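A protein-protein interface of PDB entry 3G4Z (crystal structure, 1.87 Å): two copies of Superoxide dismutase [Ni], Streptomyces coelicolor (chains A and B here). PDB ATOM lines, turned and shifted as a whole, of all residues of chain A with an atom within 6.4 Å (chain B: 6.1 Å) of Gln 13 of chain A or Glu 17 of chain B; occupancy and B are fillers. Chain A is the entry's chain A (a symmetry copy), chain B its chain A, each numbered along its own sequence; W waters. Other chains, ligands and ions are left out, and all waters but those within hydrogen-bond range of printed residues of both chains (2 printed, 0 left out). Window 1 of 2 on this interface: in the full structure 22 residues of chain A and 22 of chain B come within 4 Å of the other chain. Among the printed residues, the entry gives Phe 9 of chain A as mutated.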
ATOM      1  N   HIS A   1      14.484 -20.250 -29.639  1.00  0.00           N
ATOM      2  CA  HIS A   1      13.306 -20.741 -28.863  1.00  0.00           C
ATOM      3  C   HIS A   1      12.104 -21.016 -29.764  1.00  0.00           C
ATOM      4  O   HIS A   1      11.053 -21.468 -29.304  1.00  0.00           O
ATOM      5  CB  HIS A   1      12.944 -19.746 -27.768  1.00  0.00           C
ATOM      6  CG  HIS A   1      12.812 -18.341 -28.256  1.00  0.00           C
ATOM      7  ND1 HIS A   1      13.409 -17.275 -27.621  1.00  0.00           N
ATOM      8  CD2 HIS A   1      12.161 -17.825 -29.326  1.00  0.00           C
ATOM      9  CE1 HIS A   1      13.123 -16.163 -28.272  1.00  0.00           C
ATOM     10  NE2 HIS A   1      12.366 -16.467 -29.312  1.00  0.00           N
ATOM     11  N   CYS A   2      12.296 -20.753 -31.056  1.00  0.00           N
ATOM     12  CA  CYS A   2      11.288 -20.934 -32.110  1.00  0.00           C
ATOM     13  C   CYS A   2      11.435 -22.264 -32.879  1.00  0.00           C
ATOM     14  O   CYS A   2      10.530 -22.652 -33.617  1.00  0.00           O
ATOM     15  CB  CYS A   2      11.423 -19.787 -33.095  1.00  0.00           C
ATOM     16  SG  CYS A   2      13.124 -19.662 -33.753  1.00  0.00           S
ATOM     17  N   VAL A   8      18.484 -18.376 -30.481  1.00  0.00           N
ATOM     18  CA  VAL A   8      18.287 -17.298 -29.490  1.00  0.00           C
ATOM     19  C   VAL A   8      17.458 -17.847 -28.325  1.00  0.00           C
ATOM     20  O   VAL A   8      16.261 -18.131 -28.465  1.00  0.00           O
ATOM     21  CB  VAL A   8      17.582 -16.031 -30.048  1.00  0.00           C
ATOM     22  CG1 VAL A   8      17.474 -14.942 -28.953  1.00  0.00           C
ATOM     23  CG2 VAL A   8      18.294 -15.455 -31.253  1.00  0.00           C
ATOM     24  N   PHE A   9      18.121 -17.990 -27.189  1.00  0.00           N
ATOM     25  CA  PHE A   9      17.531 -18.512 -25.977  1.00  0.00           C
ATOM     26  C   PHE A   9      17.947 -17.609 -24.842  1.00  0.00           C
ATOM     27  O   PHE A   9      18.990 -16.998 -24.908  1.00  0.00           O
ATOM     28  CB  PHE A   9      18.022 -19.932 -25.740  1.00  0.00           C
ATOM     29  CG  PHE A   9      17.467 -20.922 -26.729  1.00  0.00           C
ATOM     30  CD1 PHE A   9      18.208 -21.289 -27.874  1.00  0.00           C
ATOM     31  CD2 PHE A   9      16.188 -21.452 -26.548  1.00  0.00           C
ATOM     32  CE1 PHE A   9      17.682 -22.209 -28.810  1.00  0.00           C
ATOM     33  CE2 PHE A   9      15.639 -22.360 -27.477  1.00  0.00           C
ATOM     34  CZ  PHE A   9      16.376 -22.730 -28.607  1.00  0.00           C
ATOM     35  N   ASP A  10      17.115 -17.527 -23.808  1.00  0.00           N
ATOM     36  CA  ASP A  10      17.480 -16.863 -22.568  1.00  0.00           C
ATOM     37  C   ASP A  10      16.451 -17.278 -21.505  1.00  0.00           C
ATOM     38  O   ASP A  10      15.261 -17.065 -21.719  1.00  0.00           O
ATOM     39  CB  ASP A  10      17.436 -15.345 -22.725  1.00  0.00           C
ATOM     40  CG  ASP A  10      18.018 -14.601 -21.525  1.00  0.00           C
ATOM     41  OD1 ASP A  10      18.178 -15.192 -20.448  1.00  0.00           O
ATOM     42  OD2 ASP A  10      18.315 -13.407 -21.678  1.00  0.00           O
ATOM     43  N   PRO A  11      16.918 -17.851 -20.380  1.00  0.00           N
ATOM     44  CA  PRO A  11      16.029 -18.260 -19.286  1.00  0.00           C
ATOM     45  C   PRO A  11      15.309 -17.058 -18.678  1.00  0.00           C
ATOM     46  O   PRO A  11      14.354 -17.253 -17.928  1.00  0.00           O
ATOM     47  CB  PRO A  11      16.983 -18.930 -18.268  1.00  0.00           C
ATOM     48  CG  PRO A  11      18.245 -19.200 -19.030  1.00  0.00           C
ATOM     49  CD  PRO A  11      18.327 -18.046 -20.006  1.00  0.00           C
ATOM     50  N   ALA A  12      15.736 -15.828 -18.995  1.00  0.00           N
ATOM     51  CA  ALA A  12      14.936 -14.628 -18.640  1.00  0.00           C
ATOM     52  C   ALA A  12      13.448 -14.726 -19.023  1.00  0.00           C
ATOM     53  O   ALA A  12      12.596 -14.134 -18.341  1.00  0.00           O
ATOM     54  CB  ALA A  12      15.542 -13.319 -19.267  1.00  0.00           C
ATOM     55  N   GLN A  13      13.149 -15.413 -20.130  1.00  0.00           N
ATOM     56  CA  GLN A  13      11.737 -15.573 -20.562  1.00  0.00           C
ATOM     57  C   GLN A  13      10.968 -16.380 -19.498  1.00  0.00           C
ATOM     58  O   GLN A  13       9.934 -15.934 -19.009  1.00  0.00           O
ATOM     59  CB  GLN A  13      11.656 -16.285 -21.902  1.00  0.00           C
ATOM     60  CG  GLN A  13      12.323 -15.495 -23.046  1.00  0.00           C
ATOM     61  CD  GLN A  13      11.925 -16.047 -24.391  1.00  0.00           C
ATOM     62  OE1 GLN A  13      12.490 -17.038 -24.876  1.00  0.00           O
ATOM     63  NE2 GLN A  13      10.933 -15.417 -24.996  1.00  0.00           N
ATOM     64  N   ALA A  14      11.516 -17.533 -19.114  1.00  0.00           N
ATOM     65  CA  ALA A  14      10.902 -18.314 -18.025  1.00  0.00           C
ATOM     66  C   ALA A  14      10.836 -17.478 -16.748  1.00  0.00           C
ATOM     67  O   ALA A  14       9.809 -17.458 -16.049  1.00  0.00           O
ATOM     68  CB  ALA A  14      11.698 -19.590 -17.750  1.00  0.00           C
ATOM     69  N   ARG A  15      11.948 -16.842 -16.403  1.00  0.00           N
ATOM     70  CA  ARG A  15      12.008 -16.072 -15.165  1.00  0.00           C
ATOM     71  C   ARG A  15      10.987 -14.962 -15.078  1.00  0.00           C
ATOM     72  O   ARG A  15      10.393 -14.776 -14.023  1.00  0.00           O
ATOM     73  CB  ARG A  15      13.398 -15.462 -14.942  1.00  0.00           C
ATOM     74  CG  ARG A  15      13.457 -14.526 -13.688  1.00  0.00           C
ATOM     75  CD  ARG A  15      14.820 -13.867 -13.479  1.00  0.00           C
ATOM     76  NE  ARG A  15      15.236 -12.990 -14.593  1.00  0.00           N
ATOM     77  CZ  ARG A  15      16.190 -13.181 -15.505  1.00  0.00           C
ATOM     78  NH1 ARG A  15      16.945 -14.262 -15.526  1.00  0.00           N
ATOM     79  NH2 ARG A  15      16.378 -12.245 -16.414  1.00  0.00           N
ATOM     80  N   ILE A  16      10.851 -14.142 -16.117  1.00  0.00           N
ATOM     81  CA  ILE A  16       9.848 -13.103 -16.073  1.00  0.00           C
ATOM     82  C   ILE A  16       8.421 -13.639 -15.879  1.00  0.00           C
ATOM     83  O   ILE A  16       7.631 -13.050 -15.116  1.00  0.00           O
ATOM     84  CB  ILE A  16       9.913 -12.130 -17.307  1.00  0.00           C
ATOM     85  CG1 ILE A  16       9.064 -10.885 -17.018  1.00  0.00           C
ATOM     86  CG2 ILE A  16       9.437 -12.830 -18.571  1.00  0.00           C
ATOM     87  CD1 ILE A  16       9.472  -9.644 -17.788  1.00  0.00           C
ATOM     88  N   GLU A  17       8.093 -14.767 -16.524  1.00  0.00           N
ATOM     89  CA  GLU A  17       6.758 -15.340 -16.369  1.00  0.00           C
ATOM     90  C   GLU A  17       6.585 -15.888 -14.940  1.00  0.00           C
ATOM     91  O   GLU A  17       5.532 -15.691 -14.310  1.00  0.00           O
ATOM     92  CB  GLU A  17       6.469 -16.383 -17.446  1.00  0.00           C
ATOM     93  CG  GLU A  17       6.462 -15.766 -18.904  1.00  0.00           C
ATOM     94  CD  GLU A  17       5.390 -14.694 -19.115  1.00  0.00           C
ATOM     95  OE1 GLU A  17       5.443 -14.018 -20.171  1.00  0.00           O
ATOM     96  OE2 GLU A  17       4.477 -14.548 -18.251  1.00  0.00           O
ATOM     97  N   ALA A  18       7.631 -16.511 -14.406  1.00  0.00           N
ATOM     98  CA  ALA A  18       7.585 -16.991 -13.016  1.00  0.00           C
ATOM     99  C   ALA A  18       7.519 -15.851 -11.984  1.00  0.00           C
ATOM    100  O   ALA A  18       6.887 -15.992 -10.942  1.00  0.00           O
ATOM    101  CB  ALA A  18       8.724 -17.920 -12.766  1.00  0.00           C
ATOM    102  N   LEU A  50       2.971 -20.531 -19.352  1.00  0.00           N
ATOM    103  CA  LEU A  50       4.016 -19.958 -20.238  1.00  0.00           C
ATOM    104  C   LEU A  50       5.459 -20.220 -19.706  1.00  0.00           C
ATOM    105  O   LEU A  50       6.405 -20.522 -20.483  1.00  0.00           O
ATOM    106  CB  LEU A  50       3.824 -18.463 -20.415  1.00  0.00           C
ATOM    107  CG  LEU A  50       2.893 -17.919 -21.492  1.00  0.00           C
ATOM    108  CD1 LEU A  50       2.652 -16.424 -21.252  1.00  0.00           C
ATOM    109  CD2 LEU A  50       3.458 -18.148 -22.916  1.00  0.00           C
ATOM    110  N   ALA A  51       5.620 -20.041 -18.408  1.00  0.00           N
ATOM    111  CA  ALA A  51       6.891 -20.307 -17.739  1.00  0.00           C
ATOM    112  C   ALA A  51       7.299 -21.743 -17.989  1.00  0.00           C
ATOM    113  O   ALA A  51       8.445 -21.981 -18.337  1.00  0.00           O
ATOM    114  CB  ALA A  51       6.804 -20.030 -16.242  1.00  0.00           C
ATOM    115  N   HIS A  54       8.528 -22.191 -21.521  1.00  0.00           N
ATOM    116  CA  HIS A  54       9.896 -21.636 -21.723  1.00  0.00           C
ATOM    117  C   HIS A  54      10.947 -22.569 -21.152  1.00  0.00           C
ATOM    118  O   HIS A  54      11.964 -22.798 -21.761  1.00  0.00           O
ATOM    119  CB  HIS A  54      10.068 -20.239 -21.118  1.00  0.00           C
ATOM    120  CG  HIS A  54       9.293 -19.168 -21.822  1.00  0.00           C
ATOM    121  ND1 HIS A  54       9.245 -19.074 -23.199  1.00  0.00           N
ATOM    122  CD2 HIS A  54       8.512 -18.164 -21.345  1.00  0.00           C
ATOM    123  CE1 HIS A  54       8.500 -18.031 -23.540  1.00  0.00           C
ATOM    124  NE2 HIS A  54       8.037 -17.469 -22.435  1.00  0.00           N
ATOM    125  N   ALA B  12      12.883  -6.629 -22.223  1.00  0.00           N
ATOM    126  CA  ALA B  12      13.604  -7.867 -22.616  1.00  0.00           C
ATOM    127  C   ALA B  12      12.732  -8.894 -23.359  1.00  0.00           C
ATOM    128  O   ALA B  12      13.249  -9.647 -24.201  1.00  0.00           O
ATOM    129  CB  ALA B  12      14.279  -8.564 -21.377  1.00  0.00           C
ATOM    130  N   GLN B  13      11.444  -8.966 -23.010  1.00  0.00           N
ATOM    131  CA  GLN B  13      10.528  -9.917 -23.688  1.00  0.00           C
ATOM    132  C   GLN B  13      10.409  -9.534 -25.176  1.00  0.00           C
ATOM    133  O   GLN B  13      10.635 -10.365 -26.051  1.00  0.00           O
ATOM    134  CB  GLN B  13       9.152  -9.902 -23.042  1.00  0.00           C
ATOM    135  CG  GLN B  13       9.170 -10.363 -21.573  1.00  0.00           C
ATOM    136  CD  GLN B  13       7.777 -10.667 -21.081  1.00  0.00           C
ATOM    137  OE1 GLN B  13       7.021  -9.768 -20.689  1.00  0.00           O
ATOM    138  NE2 GLN B  13       7.423 -11.940 -21.118  1.00  0.00           N
ATOM    139  N   ALA B  14      10.108  -8.263 -25.442  1.00  0.00           N
ATOM    140  CA  ALA B  14      10.081  -7.789 -26.837  1.00  0.00           C
ATOM    141  C   ALA B  14      11.441  -8.006 -27.497  1.00  0.00           C
ATOM    142  O   ALA B  14      11.528  -8.475 -28.644  1.00  0.00           O
ATOM    143  CB  ALA B  14       9.722  -6.304 -26.904  1.00  0.00           C
ATOM    144  N   ARG B  15      12.501  -7.606 -26.804  1.00  0.00           N
ATOM    145  CA  ARG B  15      13.840  -7.707 -27.376  1.00  0.00           C
ATOM    146  C   ARG B  15      14.244  -9.112 -27.757  1.00  0.00           C
ATOM    147  O   ARG B  15      14.835  -9.300 -28.814  1.00  0.00           O
ATOM    148  CB  ARG B  15      14.906  -7.144 -26.426  1.00  0.00           C
ATOM    149  CG  ARG B  15      16.364  -7.356 -26.956  1.00  0.00           C
ATOM    150  CD  ARG B  15      17.443  -6.849 -26.001  1.00  0.00           C
ATOM    151  NE  ARG B  15      17.444  -7.527 -24.688  1.00  0.00           N
ATOM    152  CZ  ARG B  15      17.078  -7.055 -23.496  1.00  0.00           C
ATOM    153  NH1 ARG B  15      16.637  -5.825 -23.323  1.00  0.00           N
ATOM    154  NH2 ARG B  15      17.166  -7.859 -22.454  1.00  0.00           N
ATOM    155  N   ILE B  16      14.050 -10.090 -26.876  1.00  0.00           N
ATOM    156  CA  ILE B  16      14.385 -11.447 -27.238  1.00  0.00           C
ATOM    157  C   ILE B  16      13.627 -11.954 -28.475  1.00  0.00           C
ATOM    158  O   ILE B  16      14.218 -12.639 -29.332  1.00  0.00           O
ATOM    159  CB  ILE B  16      14.239 -12.460 -26.043  1.00  0.00           C
ATOM    160  CG1 ILE B  16      14.927 -13.780 -26.408  1.00  0.00           C
ATOM    161  CG2 ILE B  16      12.773 -12.686 -25.705  1.00  0.00           C
ATOM    162  CD1 ILE B  16      15.389 -14.606 -25.223  1.00  0.00           C
ATOM    163  N   GLU B  17      12.341 -11.598 -28.599  1.00  0.00           N
ATOM    164  CA  GLU B  17      11.569 -12.032 -29.760  1.00  0.00           C
ATOM    165  C   GLU B  17      12.080 -11.321 -31.028  1.00  0.00           C
ATOM    166  O   GLU B  17      12.229 -11.949 -32.089  1.00  0.00           O
ATOM    167  CB  GLU B  17      10.069 -11.842 -29.536  1.00  0.00           C
ATOM    168  CG  GLU B  17       9.516 -12.726 -28.347  1.00  0.00           C
ATOM    169  CD  GLU B  17       9.680 -14.232 -28.568  1.00  0.00           C
ATOM    170  OE1 GLU B  17       9.451 -14.992 -27.596  1.00  0.00           O
ATOM    171  OE2 GLU B  17      10.001 -14.660 -29.715  1.00  0.00           O
ATOM    172  N   ALA B  18      12.413 -10.040 -30.903  1.00  0.00           N
ATOM    173  CA  ALA B  18      12.992  -9.306 -32.039  1.00  0.00           C
ATOM    174  C   ALA B  18      14.392  -9.808 -32.435  1.00  0.00           C
ATOM    175  O   ALA B  18      14.747  -9.800 -33.610  1.00  0.00           O
ATOM    176  CB  ALA B  18      12.973  -7.841 -31.755  1.00  0.00           C
ATOM    177  N   GLU B  19      15.192 -10.240 -31.465  1.00  0.00           N
ATOM    178  CA  GLU B  19      16.457 -10.930 -31.748  1.00  0.00           C
ATOM    179  C   GLU B  19      16.270 -12.208 -32.539  1.00  0.00           C
ATOM    180  O   GLU B  19      17.051 -12.483 -33.483  1.00  0.00           O
ATOM    181  CB  GLU B  19      17.271 -11.200 -30.474  1.00  0.00           C
ATOM    182  CG  GLU B  19      17.855  -9.891 -29.900  1.00  0.00           C
ATOM    183  CD  GLU B  19      18.504 -10.053 -28.557  1.00  0.00           C
ATOM    184  OE1 GLU B  19      18.893  -9.021 -27.961  1.00  0.00           O
ATOM    185  OE2 GLU B  19      18.621 -11.203 -28.100  1.00  0.00           O
ATOM    186  N   SER B  20      15.226 -12.966 -32.204  1.00  0.00           N
ATOM    187  CA  SER B  20      14.937 -14.173 -32.956  1.00  0.00           C
ATOM    188  C   SER B  20      14.596 -13.808 -34.391  1.00  0.00           C
ATOM    189  O   SER B  20      14.983 -14.519 -35.328  1.00  0.00           O
ATOM    190  CB  SER B  20      13.815 -14.985 -32.316  1.00  0.00           C
ATOM    191  OG  SER B  20      14.220 -15.418 -31.014  1.00  0.00           O
ATOM    192  N   VAL B  21      13.871 -12.711 -34.566  1.00  0.00           N
ATOM    193  CA  VAL B  21      13.495 -12.272 -35.918  1.00  0.00           C
ATOM    194  C   VAL B  21      14.778 -12.004 -36.728  1.00  0.00           C
ATOM    195  O   VAL B  21      14.938 -12.538 -37.853  1.00  0.00           O
ATOM    196  CB  VAL B  21      12.590 -11.060 -35.871  1.00  0.00           C
ATOM    197  CG1 VAL B  21      12.431 -10.387 -37.298  1.00  0.00           C
ATOM    198  CG2 VAL B  21      11.218 -11.467 -35.329  1.00  0.00           C
ATOM    199  N   LYS B  22      15.675 -11.184 -36.173  1.00  0.00           N
ATOM    200  CA  LYS B  22      16.933 -10.862 -36.902  1.00  0.00           C
ATOM    201  C   LYS B  22      17.780 -12.107 -37.129  1.00  0.00           C
ATOM    202  O   LYS B  22      18.335 -12.288 -38.209  1.00  0.00           O
ATOM    203  CB  LYS B  22      17.775  -9.821 -36.185  1.00  0.00           C
ATOM    204  CG  LYS B  22      18.958  -9.333 -37.067  1.00  0.00           C
ATOM    205  CD  LYS B  22      19.768  -8.291 -36.336  1.00  0.00           C
ATOM    206  CE  LYS B  22      21.032  -7.950 -37.172  1.00  0.00           C
ATOM    207  NZ  LYS B  22      22.034  -6.999 -36.536  1.00  0.00           N
ATOM    208  N   GLN B  46       5.731 -15.511 -36.687  1.00  0.00           N
ATOM    209  CA  GLN B  46       5.278 -15.734 -35.330  1.00  0.00           C
ATOM    210  C   GLN B  46       6.078 -14.925 -34.328  1.00  0.00           C
ATOM    211  O   GLN B  46       5.505 -14.292 -33.437  1.00  0.00           O
ATOM    212  CB  GLN B  46       5.422 -17.224 -34.961  1.00  0.00           C
ATOM    213  CG  GLN B  46       4.554 -18.090 -35.752  1.00  0.00           C
ATOM    214  CD  GLN B  46       4.851 -19.596 -35.600  1.00  0.00           C
ATOM    215  OE1 GLN B  46       5.991 -20.026 -35.286  1.00  0.00           O
ATOM    216  NE2 GLN B  46       3.837 -20.402 -35.879  1.00  0.00           N
ATOM    217  N   ARG B  47       7.391 -14.915 -34.459  1.00  0.00           N
ATOM    218  CA  ARG B  47       8.221 -14.218 -33.457  1.00  0.00           C
ATOM    219  C   ARG B  47       8.047 -12.705 -33.551  1.00  0.00           C
ATOM    220  O   ARG B  47       8.081 -11.976 -32.551  1.00  0.00           O
ATOM    221  CB  ARG B  47       9.693 -14.589 -33.607  1.00  0.00           C
ATOM    222  CG  ARG B  47      10.007 -16.077 -33.524  1.00  0.00           C
ATOM    223  CD  ARG B  47       9.944 -16.526 -32.102  1.00  0.00           C
ATOM    224  NE  ARG B  47       9.080 -17.681 -31.933  1.00  0.00           N
ATOM    225  CZ  ARG B  47       8.691 -18.167 -30.753  1.00  0.00           C
ATOM    226  NH1 ARG B  47       9.069 -17.587 -29.610  1.00  0.00           N
ATOM    227  NH2 ARG B  47       7.912 -19.239 -30.711  1.00  0.00           N
ATOM    228  N   ALA B  48       7.860 -12.219 -34.769  1.00  0.00           N
ATOM    229  CA  ALA B  48       7.642 -10.795 -34.944  1.00  0.00           C
ATOM    230  C   ALA B  48       6.306 -10.374 -34.347  1.00  0.00           C
ATOM    231  O   ALA B  48       6.183  -9.307 -33.751  1.00  0.00           O
ATOM    232  CB  ALA B  48       7.704 -10.415 -36.410  1.00  0.00           C
ATOM    233  N   LEU B  50       4.791 -11.884 -31.818  1.00  0.00           N
ATOM    234  CA  LEU B  50       4.977 -11.871 -30.344  1.00  0.00           C
ATOM    235  C   LEU B  50       5.692 -10.577 -29.846  1.00  0.00           C
ATOM    236  O   LEU B  50       5.339  -9.992 -28.786  1.00  0.00           O
ATOM    237  CB  LEU B  50       5.770 -13.078 -29.881  1.00  0.00           C
ATOM    238  CG  LEU B  50       5.072 -14.399 -29.582  1.00  0.00           C
ATOM    239  CD1 LEU B  50       6.120 -15.509 -29.436  1.00  0.00           C
ATOM    240  CD2 LEU B  50       4.200 -14.317 -28.304  1.00  0.00           C
ATOM    241  N   ALA B  51       6.722 -10.188 -30.576  1.00  0.00           N
ATOM    242  CA  ALA B  51       7.461  -8.961 -30.287  1.00  0.00           C
ATOM    243  C   ALA B  51       6.508  -7.786 -30.297  1.00  0.00           C
ATOM    244  O   ALA B  51       6.552  -6.980 -29.381  1.00  0.00           O
ATOM    245  CB  ALA B  51       8.592  -8.740 -31.286  1.00  0.00           C
ATOM    246  N   HIS B  54       4.358  -7.777 -27.205  1.00  0.00           N
ATOM    247  CA  HIS B  54       5.101  -7.325 -25.995  1.00  0.00           C
ATOM    248  C   HIS B  54       5.256  -5.816 -25.989  1.00  0.00           C
ATOM    249  O   HIS B  54       5.087  -5.182 -24.977  1.00  0.00           O
ATOM    250  CB  HIS B  54       6.478  -7.981 -25.861  1.00  0.00           C
ATOM    251  CG  HIS B  54       6.430  -9.446 -25.550  1.00  0.00           C
ATOM    252  ND1 HIS B  54       5.571  -9.973 -24.606  1.00  0.00           N
ATOM    253  CD2 HIS B  54       7.109 -10.499 -26.075  1.00  0.00           C
ATOM    254  CE1 HIS B  54       5.752 -11.285 -24.533  1.00  0.00           C
ATOM    255  NE2 HIS B  54       6.673 -11.628 -25.420  1.00  0.00           N
HETATM  256  O   HOH W   1       6.615 -15.086 -22.052  1.00  0.00           O
HETATM  257  O   HOH W   2       7.955 -14.078 -25.869  1.00  0.00           O
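Gln 13 of chain A touches Ile 16 of chain B, and with the chains exchanged Ile 16 of chain A touches Gln 13 of chain B.
Gln 13 of chain A touches Glu 17 of chain B, and with the chains exchanged Glu 17 of chain A touches Gln 13 of chain B.
Positions printed for both chains: 12, 13, 14, 15, 16, 17, 18, 50, 51 and 54.
Of the 14 pairs that touch across the chains among the printed residues, 4 have their exchanged pair printed and touching as well.
The side-chain carboxylate (OE1) of Glu 17 of chain A is in hydrogen-bond range of the side-chain amide nitrogen (NE2) of Gln 13 of chain B (3.0 Å).
NE2 of His 1 of chain A is in hydrogen-bond range of OE2 of Glu 17 of chain B.
The guanidinium group (NH1) of Arg 47 of chain B lies close to a ring nitrogen (NE2) of His 1 of chain A.
The side-chain hydroxyl (OG) of Ser 20 of chain B lies within hydrogen-bond range of a ring nitrogen (NE2) of His 1 of chain A, at 2.7 Å.
NE2 of Gln 13 of chain A sits at hydrogen-bond distance from OE1 of Glu 17 of chain B (3.0 Å).
Water W2 lies within hydrogen-bond range of OE1 of Glu 17 of chain B, NE2 of His 54 of chain B and NE2 of Gln 13 of chain A.
Water W1 lies within hydrogen-bond range of OE1 of Glu 17 of chain A, NE2 of His 54 of chain A and NE2 of Gln 13 of chain B.
A ring nitrogen (ND1) of His 1 of chain A is in hydrogen-bond range of the side-chain amide oxygen of Gln 13 of chain A (2.9 Å).
A ring nitrogen (ND1) of His 1 of chain A is in hydrogen-bond range of the backbone carbonyl oxygen (O) of Val 8 of chain A (3.1 Å).
The side-chain carboxylate (OD1) of Asp 10 of chain A sits at hydrogen-bond distance from the backbone NH (N) of Ala 12 of chain A (2.9 Å).
NE of Arg 15 of chain B is in salt-bridge range of OE1 of Glu 19 of chain B (3.9 Å).
The side-chain hydroxyl (OG) of Ser 20 of chain B lies within hydrogen-bond range of the backbone carbonyl oxygen (O) of Ile 16 of chain B (3.2 Å).
OE2 of Glu 17 of chain B is in salt-bridge range of NH1 of Arg 47 of chain B (3.1 Å).
Among the printed residues, pairs that only touch across the chains: Asp 10 of chain A with Ile 16 of chain B (3.3 Å), Cys 2 of chain A with Arg 47 of chain B (3.4 Å), Ile 16 of chain A with Gln 13 of chain B (3.4 Å), Gln 13 of chain A with Ile 16 of chain B (3.4 Å), His 1 of chain A with Ile 16 of chain B (3.5 Å), Val 8 of chain A with Ser 20 of chain B (3.6 Å), Val 8 of chain A with Ile 16 of chain B (3.8 Å), Val 8 of chain A with Glu 19 of chain B (3.9 Å) and Phe 9 of chain A with Ile 16 of chain B (3.96 Å).
Printed residues of chain A that touch a printed residue of chain B: His 1, Cys 2, Val 8, Phe 9, Asp 10, Gln 13, Ile 16 and Glu 17.
Hydrophobic or aromatic side chains of chain A within 4 Å of the printed part of chain B: His 1, Val 8 and Ile 16.
Of the 17 printed residues of chain B, 6 touch a printed residue of chain A.
Hydrophobic or aromatic side chains of chain B that line the printed part of chain A: Ile 16.
Among the printed residues, no Asp or Glu carboxylate lies within 4 Å of a Lys or Arg side-chain nitrogen of the other chain.
Gln 13 of chain A touches just these residues of chain B: Ile 16 and Glu 17.
Glu 17 of chain B touches just these residues of chain A: His 1 (3.0 Å) and Gln 13 (3.0 Å).
Printed residues of chain A within 4 Å of Ser 20 of chain B: His 1 and Val 8.
Of the printed residues of chain A, Ile 16 of chain B touches His 1, Val 8, Phe 9, Asp 10 and Gln 13.
Printed residues of chain B within 4 Å of Phe 9 of chain A: Ile 16.
Of the printed residues of chain B, His 1 of chain A touches Ile 16, Glu 17, Ser 20 and Arg 47.
Of the printed residues of chain A, Gln 13 of chain B touches Ile 16 and Glu 17.
His 54 of chain B touches none of the printed residues of chain A.
The nearest residue of chain B that does not touch Gln 13 of chain A is Gln 13 of chain B (5.2 Å).
The nearest residue of chain A that does not touch Glu 17 of chain B is His 54 of chain A (5.2 Å).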
